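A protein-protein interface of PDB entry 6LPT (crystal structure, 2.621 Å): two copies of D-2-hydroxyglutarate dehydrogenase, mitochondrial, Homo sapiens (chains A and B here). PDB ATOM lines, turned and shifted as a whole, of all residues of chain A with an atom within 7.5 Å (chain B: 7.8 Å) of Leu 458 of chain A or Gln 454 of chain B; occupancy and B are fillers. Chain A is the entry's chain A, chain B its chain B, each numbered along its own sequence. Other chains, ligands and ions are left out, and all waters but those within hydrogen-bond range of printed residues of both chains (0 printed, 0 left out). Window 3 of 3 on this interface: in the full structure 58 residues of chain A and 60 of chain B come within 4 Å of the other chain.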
ATOM      1  N   LEU A 184     -10.281  22.932  15.167  1.00  0.00           N
ATOM      2  CA  LEU A 184     -11.592  22.312  15.035  1.00  0.00           C
ATOM      3  C   LEU A 184     -12.512  23.141  14.140  1.00  0.00           C
ATOM      4  O   LEU A 184     -12.215  24.282  13.774  1.00  0.00           O
ATOM      5  CB  LEU A 184     -12.221  22.120  16.413  1.00  0.00           C
ATOM      6  CG  LEU A 184     -11.356  21.338  17.404  1.00  0.00           C
ATOM      7  CD1 LEU A 184     -12.046  21.229  18.756  1.00  0.00           C
ATOM      8  CD2 LEU A 184     -11.016  19.960  16.855  1.00  0.00           C
ATOM      9  N   TYR A 203      -7.196  11.179  28.299  1.00  0.00           N
ATOM     10  CA  TYR A 203      -7.447  10.504  27.034  1.00  0.00           C
ATOM     11  C   TYR A 203      -6.451  10.978  25.985  1.00  0.00           C
ATOM     12  O   TYR A 203      -6.057  12.147  25.955  1.00  0.00           O
ATOM     13  CB  TYR A 203      -8.875  10.750  26.541  1.00  0.00           C
ATOM     14  CG  TYR A 203      -9.992  10.415  27.508  1.00  0.00           C
ATOM     15  CD1 TYR A 203      -9.829   9.451  28.494  1.00  0.00           C
ATOM     16  CD2 TYR A 203     -11.231  11.037  27.398  1.00  0.00           C
ATOM     17  CE1 TYR A 203     -10.858   9.138  29.364  1.00  0.00           C
ATOM     18  CE2 TYR A 203     -12.264  10.732  28.258  1.00  0.00           C
ATOM     19  CZ  TYR A 203     -12.075   9.783  29.241  1.00  0.00           C
ATOM     20  OH  TYR A 203     -13.110   9.480  30.098  1.00  0.00           O
ATOM     21  N   LEU A 208      -7.623  10.506  17.837  1.00  0.00           N
ATOM     22  CA  LEU A 208      -8.804  10.739  17.006  1.00  0.00           C
ATOM     23  C   LEU A 208      -8.469  11.381  15.671  1.00  0.00           C
ATOM     24  O   LEU A 208      -9.151  11.124  14.674  1.00  0.00           O
ATOM     25  CB  LEU A 208      -9.802  11.642  17.734  1.00  0.00           C
ATOM     26  CG  LEU A 208     -10.633  11.134  18.893  1.00  0.00           C
ATOM     27  CD1 LEU A 208     -11.478  12.248  19.449  1.00  0.00           C
ATOM     28  CD2 LEU A 208     -11.562  10.149  18.241  1.00  0.00           C
ATOM     29  N   LEU A 216     -12.579  15.652  11.152  1.00  0.00           N
ATOM     30  CA  LEU A 216     -12.728  16.002  12.557  1.00  0.00           C
ATOM     31  C   LEU A 216     -11.949  17.247  12.950  1.00  0.00           C
ATOM     32  O   LEU A 216     -12.147  17.757  14.060  1.00  0.00           O
ATOM     33  CB  LEU A 216     -12.285  14.828  13.443  1.00  0.00           C
ATOM     34  CG  LEU A 216     -13.040  13.510  13.256  1.00  0.00           C
ATOM     35  CD1 LEU A 216     -12.512  12.449  14.209  1.00  0.00           C
ATOM     36  CD2 LEU A 216     -14.533  13.719  13.457  1.00  0.00           C
ATOM     37  N   MET A 452     -18.582   6.232  14.917  1.00  0.00           N
ATOM     38  CA  MET A 452     -17.846   7.178  14.077  1.00  0.00           C
ATOM     39  C   MET A 452     -18.706   8.383  13.713  1.00  0.00           C
ATOM     40  O   MET A 452     -18.260   9.536  13.790  1.00  0.00           O
ATOM     41  CB  MET A 452     -17.338   6.493  12.807  1.00  0.00           C
ATOM     42  CG  MET A 452     -16.316   5.397  13.023  1.00  0.00           C
ATOM     43  SD  MET A 452     -15.725   4.758  11.442  1.00  0.00           S
ATOM     44  CE  MET A 452     -14.883   3.265  11.955  1.00  0.00           C
ATOM     45  N   GLN A 453     -19.945   8.126  13.287  1.00  0.00           N
ATOM     46  CA  GLN A 453     -20.854   9.220  12.958  1.00  0.00           C
ATOM     47  C   GLN A 453     -21.155  10.086  14.178  1.00  0.00           C
ATOM     48  O   GLN A 453     -21.263  11.315  14.066  1.00  0.00           O
ATOM     49  CB  GLN A 453     -22.145   8.670  12.352  1.00  0.00           C
ATOM     50  CG  GLN A 453     -23.086   9.743  11.818  1.00  0.00           C
ATOM     51  CD  GLN A 453     -22.450  10.601  10.737  1.00  0.00           C
ATOM     52  OE1 GLN A 453     -22.275  11.810  10.911  1.00  0.00           O
ATOM     53  NE2 GLN A 453     -22.105   9.981   9.613  1.00  0.00           N
ATOM     54  N   GLN A 454     -21.265   9.469  15.357  1.00  0.00           N
ATOM     55  CA  GLN A 454     -21.486  10.253  16.572  1.00  0.00           C
ATOM     56  C   GLN A 454     -20.305  11.164  16.882  1.00  0.00           C
ATOM     57  O   GLN A 454     -20.493  12.321  17.284  1.00  0.00           O
ATOM     58  CB  GLN A 454     -21.740   9.327  17.762  1.00  0.00           C
ATOM     59  CG  GLN A 454     -23.006   8.500  17.690  1.00  0.00           C
ATOM     60  CD  GLN A 454     -23.125   7.550  18.865  1.00  0.00           C
ATOM     61  OE1 GLN A 454     -22.878   6.351  18.738  1.00  0.00           O
ATOM     62  NE2 GLN A 454     -23.489   8.088  20.023  1.00  0.00           N
ATOM     63  N   LEU A 455     -19.082  10.673  16.682  1.00  0.00           N
ATOM     64  CA  LEU A 455     -17.915  11.527  16.895  1.00  0.00           C
ATOM     65  C   LEU A 455     -17.869  12.667  15.888  1.00  0.00           C
ATOM     66  O   LEU A 455     -17.545  13.807  16.246  1.00  0.00           O
ATOM     67  CB  LEU A 455     -16.625  10.711  16.833  1.00  0.00           C
ATOM     68  CG  LEU A 455     -16.380   9.755  18.000  1.00  0.00           C
ATOM     69  CD1 LEU A 455     -15.289   8.764  17.650  1.00  0.00           C
ATOM     70  CD2 LEU A 455     -16.022  10.527  19.259  1.00  0.00           C
ATOM     71  N   LYS A 456     -18.164  12.371  14.619  1.00  0.00           N
ATOM     72  CA  LYS A 456     -18.253  13.428  13.616  1.00  0.00           C
ATOM     73  C   LYS A 456     -19.255  14.500  14.029  1.00  0.00           C
ATOM     74  O   LYS A 456     -18.979  15.700  13.911  1.00  0.00           O
ATOM     75  CB  LYS A 456     -18.638  12.828  12.264  1.00  0.00           C
ATOM     76  CG  LYS A 456     -18.940  13.831  11.160  1.00  0.00           C
ATOM     77  CD  LYS A 456     -17.771  14.763  10.896  1.00  0.00           C
ATOM     78  CE  LYS A 456     -18.126  15.777   9.821  1.00  0.00           C
ATOM     79  NZ  LYS A 456     -16.925  16.500   9.312  1.00  0.00           N
ATOM     80  N   ALA A 457     -20.428  14.083  14.515  1.00  0.00           N
ATOM     81  CA  ALA A 457     -21.445  15.041  14.945  1.00  0.00           C
ATOM     82  C   ALA A 457     -21.012  15.844  16.169  1.00  0.00           C
ATOM     83  O   ALA A 457     -21.359  17.025  16.286  1.00  0.00           O
ATOM     84  CB  ALA A 457     -22.758  14.317  15.231  1.00  0.00           C
ATOM     85  N   LEU A 458     -20.257  15.231  17.084  1.00  0.00           N
ATOM     86  CA  LEU A 458     -19.752  15.966  18.242  1.00  0.00           C
ATOM     87  C   LEU A 458     -18.708  17.004  17.839  1.00  0.00           C
ATOM     88  O   LEU A 458     -18.771  18.162  18.271  1.00  0.00           O
ATOM     89  CB  LEU A 458     -19.178  14.995  19.275  1.00  0.00           C
ATOM     90  CG  LEU A 458     -18.411  15.592  20.461  1.00  0.00           C
ATOM     91  CD1 LEU A 458     -19.273  16.579  21.229  1.00  0.00           C
ATOM     92  CD2 LEU A 458     -17.909  14.491  21.382  1.00  0.00           C
ATOM     93  N   LEU A 459     -17.738  16.612  17.013  1.00  0.00           N
ATOM     94  CA  LEU A 459     -16.619  17.499  16.705  1.00  0.00           C
ATOM     95  C   LEU A 459     -16.950  18.516  15.619  1.00  0.00           C
ATOM     96  O   LEU A 459     -16.354  19.599  15.593  1.00  0.00           O
ATOM     97  CB  LEU A 459     -15.386  16.688  16.307  1.00  0.00           C
ATOM     98  CG  LEU A 459     -14.688  15.964  17.458  1.00  0.00           C
ATOM     99  CD1 LEU A 459     -13.685  14.950  16.930  1.00  0.00           C
ATOM    100  CD2 LEU A 459     -14.001  16.967  18.371  1.00  0.00           C
ATOM    101  N   ASP A 460     -17.885  18.203  14.722  1.00  0.00           N
ATOM    102  CA  ASP A 460     -18.217  19.073  13.592  1.00  0.00           C
ATOM    103  C   ASP A 460     -19.714  18.957  13.324  1.00  0.00           C
ATOM    104  O   ASP A 460     -20.149  18.350  12.337  1.00  0.00           O
ATOM    105  CB  ASP A 460     -17.373  18.695  12.370  1.00  0.00           C
ATOM    106  CG  ASP A 460     -17.737  19.476  11.125  1.00  0.00           C
ATOM    107  OD1 ASP A 460     -18.283  20.594  11.248  1.00  0.00           O
ATOM    108  OD2 ASP A 460     -17.456  18.964  10.017  1.00  0.00           O
ATOM    109  N   PRO A 461     -20.540  19.511  14.220  1.00  0.00           N
ATOM    110  CA  PRO A 461     -21.999  19.375  14.060  1.00  0.00           C
ATOM    111  C   PRO A 461     -22.554  19.951  12.768  1.00  0.00           C
ATOM    112  O   PRO A 461     -23.544  19.419  12.251  1.00  0.00           O
ATOM    113  CB  PRO A 461     -22.558  20.117  15.284  1.00  0.00           C
ATOM    114  CG  PRO A 461     -21.431  20.972  15.776  1.00  0.00           C
ATOM    115  CD  PRO A 461     -20.184  20.225  15.456  1.00  0.00           C
ATOM    116  N   LYS A 462     -21.964  21.019  12.229  1.00  0.00           N
ATOM    117  CA  LYS A 462     -22.434  21.546  10.952  1.00  0.00           C
ATOM    118  C   LYS A 462     -21.939  20.739   9.762  1.00  0.00           C
ATOM    119  O   LYS A 462     -22.456  20.918   8.654  1.00  0.00           O
ATOM    120  CB  LYS A 462     -22.028  23.014  10.781  1.00  0.00           C
ATOM    121  CG  LYS A 462     -22.629  23.965  11.806  1.00  0.00           C
ATOM    122  CD  LYS A 462     -22.437  25.414  11.373  1.00  0.00           C
ATOM    123  CE  LYS A 462     -23.007  26.388  12.391  1.00  0.00           C
ATOM    124  NZ  LYS A 462     -23.128  27.762  11.826  1.00  0.00           N
ATOM    125  N   LEU B 216     -14.730   5.068  29.655  1.00  0.00           N
ATOM    126  CA  LEU B 216     -15.439   5.129  28.385  1.00  0.00           C
ATOM    127  C   LEU B 216     -16.010   3.786  27.954  1.00  0.00           C
ATOM    128  O   LEU B 216     -16.835   3.746  27.036  1.00  0.00           O
ATOM    129  CB  LEU B 216     -14.521   5.671  27.281  1.00  0.00           C
ATOM    130  CG  LEU B 216     -13.993   7.089  27.502  1.00  0.00           C
ATOM    131  CD1 LEU B 216     -13.063   7.502  26.373  1.00  0.00           C
ATOM    132  CD2 LEU B 216     -15.151   8.057  27.637  1.00  0.00           C
ATOM    133  N   GLY B 447      -8.662  23.312  27.074  1.00  0.00           N
ATOM    134  CA  GLY B 447      -9.462  22.848  25.946  1.00  0.00           C
ATOM    135  C   GLY B 447      -9.406  21.345  25.734  1.00  0.00           C
ATOM    136  O   GLY B 447     -10.422  20.714  25.421  1.00  0.00           O
ATOM    137  N   ALA B 448      -8.232  20.743  25.934  1.00  0.00           N
ATOM    138  CA  ALA B 448      -8.139  19.288  25.861  1.00  0.00           C
ATOM    139  C   ALA B 448      -8.986  18.623  26.941  1.00  0.00           C
ATOM    140  O   ALA B 448      -9.708  17.654  26.670  1.00  0.00           O
ATOM    141  CB  ALA B 448      -6.678  18.856  25.980  1.00  0.00           C
ATOM    142  N   LEU B 449      -8.888  19.112  28.180  1.00  0.00           N
ATOM    143  CA  LEU B 449      -9.694  18.548  29.260  1.00  0.00           C
ATOM    144  C   LEU B 449     -11.186  18.674  28.966  1.00  0.00           C
ATOM    145  O   LEU B 449     -11.969  17.757  29.256  1.00  0.00           O
ATOM    146  CB  LEU B 449      -9.347  19.250  30.573  1.00  0.00           C
ATOM    147  CG  LEU B 449      -7.913  19.082  31.077  1.00  0.00           C
ATOM    148  CD1 LEU B 449      -7.674  19.897  32.339  1.00  0.00           C
ATOM    149  CD2 LEU B 449      -7.616  17.614  31.332  1.00  0.00           C
ATOM    150  N   GLN B 450     -11.589  19.773  28.325  1.00  0.00           N
ATOM    151  CA  GLN B 450     -12.997  19.941  27.991  1.00  0.00           C
ATOM    152  C   GLN B 450     -13.422  18.936  26.928  1.00  0.00           C
ATOM    153  O   GLN B 450     -14.513  18.355  27.015  1.00  0.00           O
ATOM    154  CB  GLN B 450     -13.255  21.382  27.545  1.00  0.00           C
ATOM    155  CG  GLN B 450     -14.714  21.726  27.310  1.00  0.00           C
ATOM    156  CD  GLN B 450     -14.893  23.046  26.583  1.00  0.00           C
ATOM    157  OE1 GLN B 450     -15.278  23.071  25.415  1.00  0.00           O
ATOM    158  NE2 GLN B 450     -14.613  24.151  27.271  1.00  0.00           N
ATOM    159  N   LEU B 451     -12.601  18.756  25.887  1.00  0.00           N
ATOM    160  CA  LEU B 451     -12.937  17.767  24.869  1.00  0.00           C
ATOM    161  C   LEU B 451     -13.034  16.367  25.474  1.00  0.00           C
ATOM    162  O   LEU B 451     -13.891  15.567  25.078  1.00  0.00           O
ATOM    163  CB  LEU B 451     -11.913  17.791  23.734  1.00  0.00           C
ATOM    164  CG  LEU B 451     -12.155  16.742  22.645  1.00  0.00           C
ATOM    165  CD1 LEU B 451     -13.550  16.900  22.056  1.00  0.00           C
ATOM    166  CD2 LEU B 451     -11.099  16.838  21.562  1.00  0.00           C
ATOM    167  N   MET B 452     -12.169  16.061  26.452  1.00  0.00           N
ATOM    168  CA  MET B 452     -12.277  14.789  27.165  1.00  0.00           C
ATOM    169  C   MET B 452     -13.608  14.668  27.896  1.00  0.00           C
ATOM    170  O   MET B 452     -14.242  13.603  27.890  1.00  0.00           O
ATOM    171  CB  MET B 452     -11.122  14.645  28.157  1.00  0.00           C
ATOM    172  CG  MET B 452      -9.760  14.486  27.526  1.00  0.00           C
ATOM    173  SD  MET B 452      -8.455  14.543  28.770  1.00  0.00           S
ATOM    174  CE  MET B 452      -9.166  13.523  30.064  1.00  0.00           C
ATOM    175  N   GLN B 453     -14.054  15.758  28.524  1.00  0.00           N
ATOM    176  CA  GLN B 453     -15.339  15.726  29.220  1.00  0.00           C
ATOM    177  C   GLN B 453     -16.487  15.498  28.243  1.00  0.00           C
ATOM    178  O   GLN B 453     -17.448  14.780  28.550  1.00  0.00           O
ATOM    179  CB  GLN B 453     -15.552  17.007  30.023  1.00  0.00           C
ATOM    180  CG  GLN B 453     -14.491  17.242  31.085  1.00  0.00           C
ATOM    181  CD  GLN B 453     -14.835  16.593  32.418  1.00  0.00           C
ATOM    182  OE1 GLN B 453     -15.720  15.739  32.493  1.00  0.00           O
ATOM    183  NE2 GLN B 453     -14.122  16.984  33.474  1.00  0.00           N
ATOM    184  N   GLN B 454     -16.405  16.111  27.061  1.00  0.00           N
ATOM    185  CA  GLN B 454     -17.429  15.901  26.038  1.00  0.00           C
ATOM    186  C   GLN B 454     -17.435  14.461  25.536  1.00  0.00           C
ATOM    187  O   GLN B 454     -18.504  13.891  25.285  1.00  0.00           O
ATOM    188  CB  GLN B 454     -17.187  16.854  24.869  1.00  0.00           C
ATOM    189  CG  GLN B 454     -17.362  18.318  25.209  1.00  0.00           C
ATOM    190  CD  GLN B 454     -16.890  19.225  24.093  1.00  0.00           C
ATOM    191  OE1 GLN B 454     -17.032  18.898  22.915  1.00  0.00           O
ATOM    192  NE2 GLN B 454     -16.319  20.367  24.457  1.00  0.00           N
ATOM    193  N   LEU B 455     -16.254  13.858  25.382  1.00  0.00           N
ATOM    194  CA  LEU B 455     -16.189  12.443  25.015  1.00  0.00           C
ATOM    195  C   LEU B 455     -16.862  11.578  26.073  1.00  0.00           C
ATOM    196  O   LEU B 455     -17.628  10.659  25.749  1.00  0.00           O
ATOM    197  CB  LEU B 455     -14.739  12.012  24.805  1.00  0.00           C
ATOM    198  CG  LEU B 455     -14.089  12.561  23.536  1.00  0.00           C
ATOM    199  CD1 LEU B 455     -12.659  12.084  23.431  1.00  0.00           C
ATOM    200  CD2 LEU B 455     -14.887  12.162  22.304  1.00  0.00           C
ATOM    201  N   LYS B 456     -16.580  11.863  27.345  1.00  0.00           N
ATOM    202  CA  LYS B 456     -17.211  11.138  28.444  1.00  0.00           C
ATOM    203  C   LYS B 456     -18.730  11.267  28.390  1.00  0.00           C
ATOM    204  O   LYS B 456     -19.455  10.277  28.540  1.00  0.00           O
ATOM    205  CB  LYS B 456     -16.675  11.670  29.775  1.00  0.00           C
ATOM    206  CG  LYS B 456     -17.326  11.092  31.022  1.00  0.00           C
ATOM    207  CD  LYS B 456     -17.117   9.596  31.165  1.00  0.00           C
ATOM    208  CE  LYS B 456     -17.844   9.080  32.399  1.00  0.00           C
ATOM    209  NZ  LYS B 456     -17.540   7.657  32.692  1.00  0.00           N
ATOM    210  N   ALA B 457     -19.225  12.489  28.183  1.00  0.00           N
ATOM    211  CA  ALA B 457     -20.668  12.707  28.104  1.00  0.00           C
ATOM    212  C   ALA B 457     -21.297  11.957  26.933  1.00  0.00           C
ATOM    213  O   ALA B 457     -22.398  11.407  27.062  1.00  0.00           O
ATOM    214  CB  ALA B 457     -20.967  14.201  27.995  1.00  0.00           C
ATOM    215  N   LEU B 458     -20.624  11.932  25.779  1.00  0.00           N
ATOM    216  CA  LEU B 458     -21.127  11.160  24.643  1.00  0.00           C
ATOM    217  C   LEU B 458     -21.187   9.668  24.953  1.00  0.00           C
ATOM    218  O   LEU B 458     -22.197   9.008  24.686  1.00  0.00           O
ATOM    219  CB  LEU B 458     -20.258  11.410  23.412  1.00  0.00           C
ATOM    220  CG  LEU B 458     -20.617  10.603  22.161  1.00  0.00           C
ATOM    221  CD1 LEU B 458     -21.960  11.034  21.591  1.00  0.00           C
ATOM    222  CD2 LEU B 458     -19.516  10.720  21.119  1.00  0.00           C
ATOM    223  N   LEU B 459     -20.116   9.114  25.516  1.00  0.00           N
ATOM    224  CA  LEU B 459     -20.030   7.664  25.656  1.00  0.00           C
ATOM    225  C   LEU B 459     -20.667   7.141  26.935  1.00  0.00           C
ATOM    226  O   LEU B 459     -21.149   6.002  26.957  1.00  0.00           O
ATOM    227  CB  LEU B 459     -18.570   7.214  25.587  1.00  0.00           C
ATOM    228  CG  LEU B 459     -17.985   7.212  24.175  1.00  0.00           C
ATOM    229  CD1 LEU B 459     -16.472   7.153  24.218  1.00  0.00           C
ATOM    230  CD2 LEU B 459     -18.546   6.048  23.368  1.00  0.00           C
ATOM    231  N   ASP B 460     -20.687   7.940  27.997  1.00  0.00           N
ATOM    232  CA  ASP B 460     -21.271   7.541  29.279  1.00  0.00           C
ATOM    233  C   ASP B 460     -22.014   8.735  29.864  1.00  0.00           C
ATOM    234  O   ASP B 460     -21.570   9.351  30.840  1.00  0.00           O
ATOM    235  CB  ASP B 460     -20.180   7.026  30.224  1.00  0.00           C
ATOM    236  CG  ASP B 460     -20.722   6.578  31.566  1.00  0.00           C
ATOM    237  OD1 ASP B 460     -21.942   6.343  31.678  1.00  0.00           O
ATOM    238  OD2 ASP B 460     -19.914   6.448  32.510  1.00  0.00           O
ATOM    239  N   PRO B 461     -23.152   9.108  29.267  1.00  0.00           N
ATOM    240  CA  PRO B 461     -23.882  10.287  29.769  1.00  0.00           C
ATOM    241  C   PRO B 461     -24.368  10.152  31.203  1.00  0.00           C
ATOM    242  O   PRO B 461     -24.480  11.168  31.901  1.00  0.00           O
ATOM    243  CB  PRO B 461     -25.060  10.420  28.790  1.00  0.00           C
ATOM    244  CG  PRO B 461     -25.161   9.108  28.091  1.00  0.00           C
ATOM    245  CD  PRO B 461     -23.790   8.514  28.080  1.00  0.00           C
ATOM    246  N   LEU B 471     -11.011  12.203  34.923  1.00  0.00           N
ATOM    247  CA  LEU B 471     -11.123  13.572  34.452  1.00  0.00           C
ATOM    248  C   LEU B 471     -11.316  14.526  35.622  1.00  0.00           C
ATOM    249  O   LEU B 471     -11.671  14.100  36.725  1.00  0.00           O
ATOM    250  CB  LEU B 471     -12.312  13.696  33.490  1.00  0.00           C
ATOM    251  CG  LEU B 471     -12.416  12.698  32.336  1.00  0.00           C
ATOM    252  CD1 LEU B 471     -13.391  11.579  32.673  1.00  0.00           C
ATOM    253  CD2 LEU B 471     -12.830  13.406  31.061  1.00  0.00           C
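Leu 458 of chain A touches just these residues of chain B: Gln 454 and Leu 455. Gln 454 of chain B touches one residue of chain A. No residue of chain B comes within 4 Å of Ala 457 of chain A. Printed residues of chain B within 4 Å of Leu 459 of chain A: Leu 451 (3.7 Å). Of the printed residues of chain B, Gln 454 of chain A touches Leu 458. Leu 459 of chain B touches none of the printed residues of chain A. Ala 457 of chain B touches none of the printed residues of chain A. The nearest residue of chain B that does not touch Leu 458 of chain A is Leu 458 of chain B (4.1 Å). The nearest residue of chain A that does not touch Gln 454 of chain B is Leu 459 of chain A (5.8 Å). The nearest printed residue of chain A that does not touch Leu 455 of chain B is Leu 208 of chain A (4.2 Å).
Of the 15 printed residues of chain A, 5 touch a printed residue of chain B. Printed residues of chain A that touch a printed residue of chain B: Tyr 203, Gln 454, Leu 455, Leu 458 and Leu 459. Hydrophobic or aromatic side chains of chain A that line the printed part of chain B: Tyr 203, Leu 455, Leu 458 and Leu 459. Of the 17 printed residues of chain B, 7 touch a printed residue of chain A. Hydrophobic or aromatic side chains of chain B within 4 Å of the printed part of chain A: Leu 216, Leu 451, Met 452, Leu 455, Leu 458 and Leu 471.
Gln 454 of chain A touches Leu 458 of chain B, and with the chains exchanged Leu 458 of chain A touches Gln 454 of chain B. Leu 455 of chain A touches its own counterpart, Leu 455 of chain B. Leu 455 of chain A touches Leu 458 of chain B, and with the chains exchanged Leu 458 of chain A touches Leu 455 of chain B. Positions printed for both chains: 216, 452, 453, 454, 455, 456, 457, 458, 459, 460 and 461. Of the 9 pairs that touch across the chains among the printed residues, 5 have their exchanged pair printed and touching as well.
Leu 216 of chain B touches Tyr 203 of chain A. Tyr 203 of chain A touches Leu 471 of chain B. Gln 454 of chain A touches Leu 458 of chain B. Leu 455 of chain A touches Leu 455 of chain B. Leu 455 of chain A touches Leu 458 of chain B (CD2 to CD2, 3.96 Å). Gln 454 of chain B touches Leu 458 of chain A. Leu 458 of chain A touches Leu 455 of chain B. CD2 of Leu 459 of chain A touches CD1 of Leu 451 of chain B (3.7 Å).
The side-chain sulfur of Met 452 of chain B sits close to the backbone NH of Tyr 203 of chain A (3.6 Å).
OE1 of Gln 450 of chain B sits at hydrogen-bond distance from NE2 of Gln 454 of chain B (3.1 Å).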
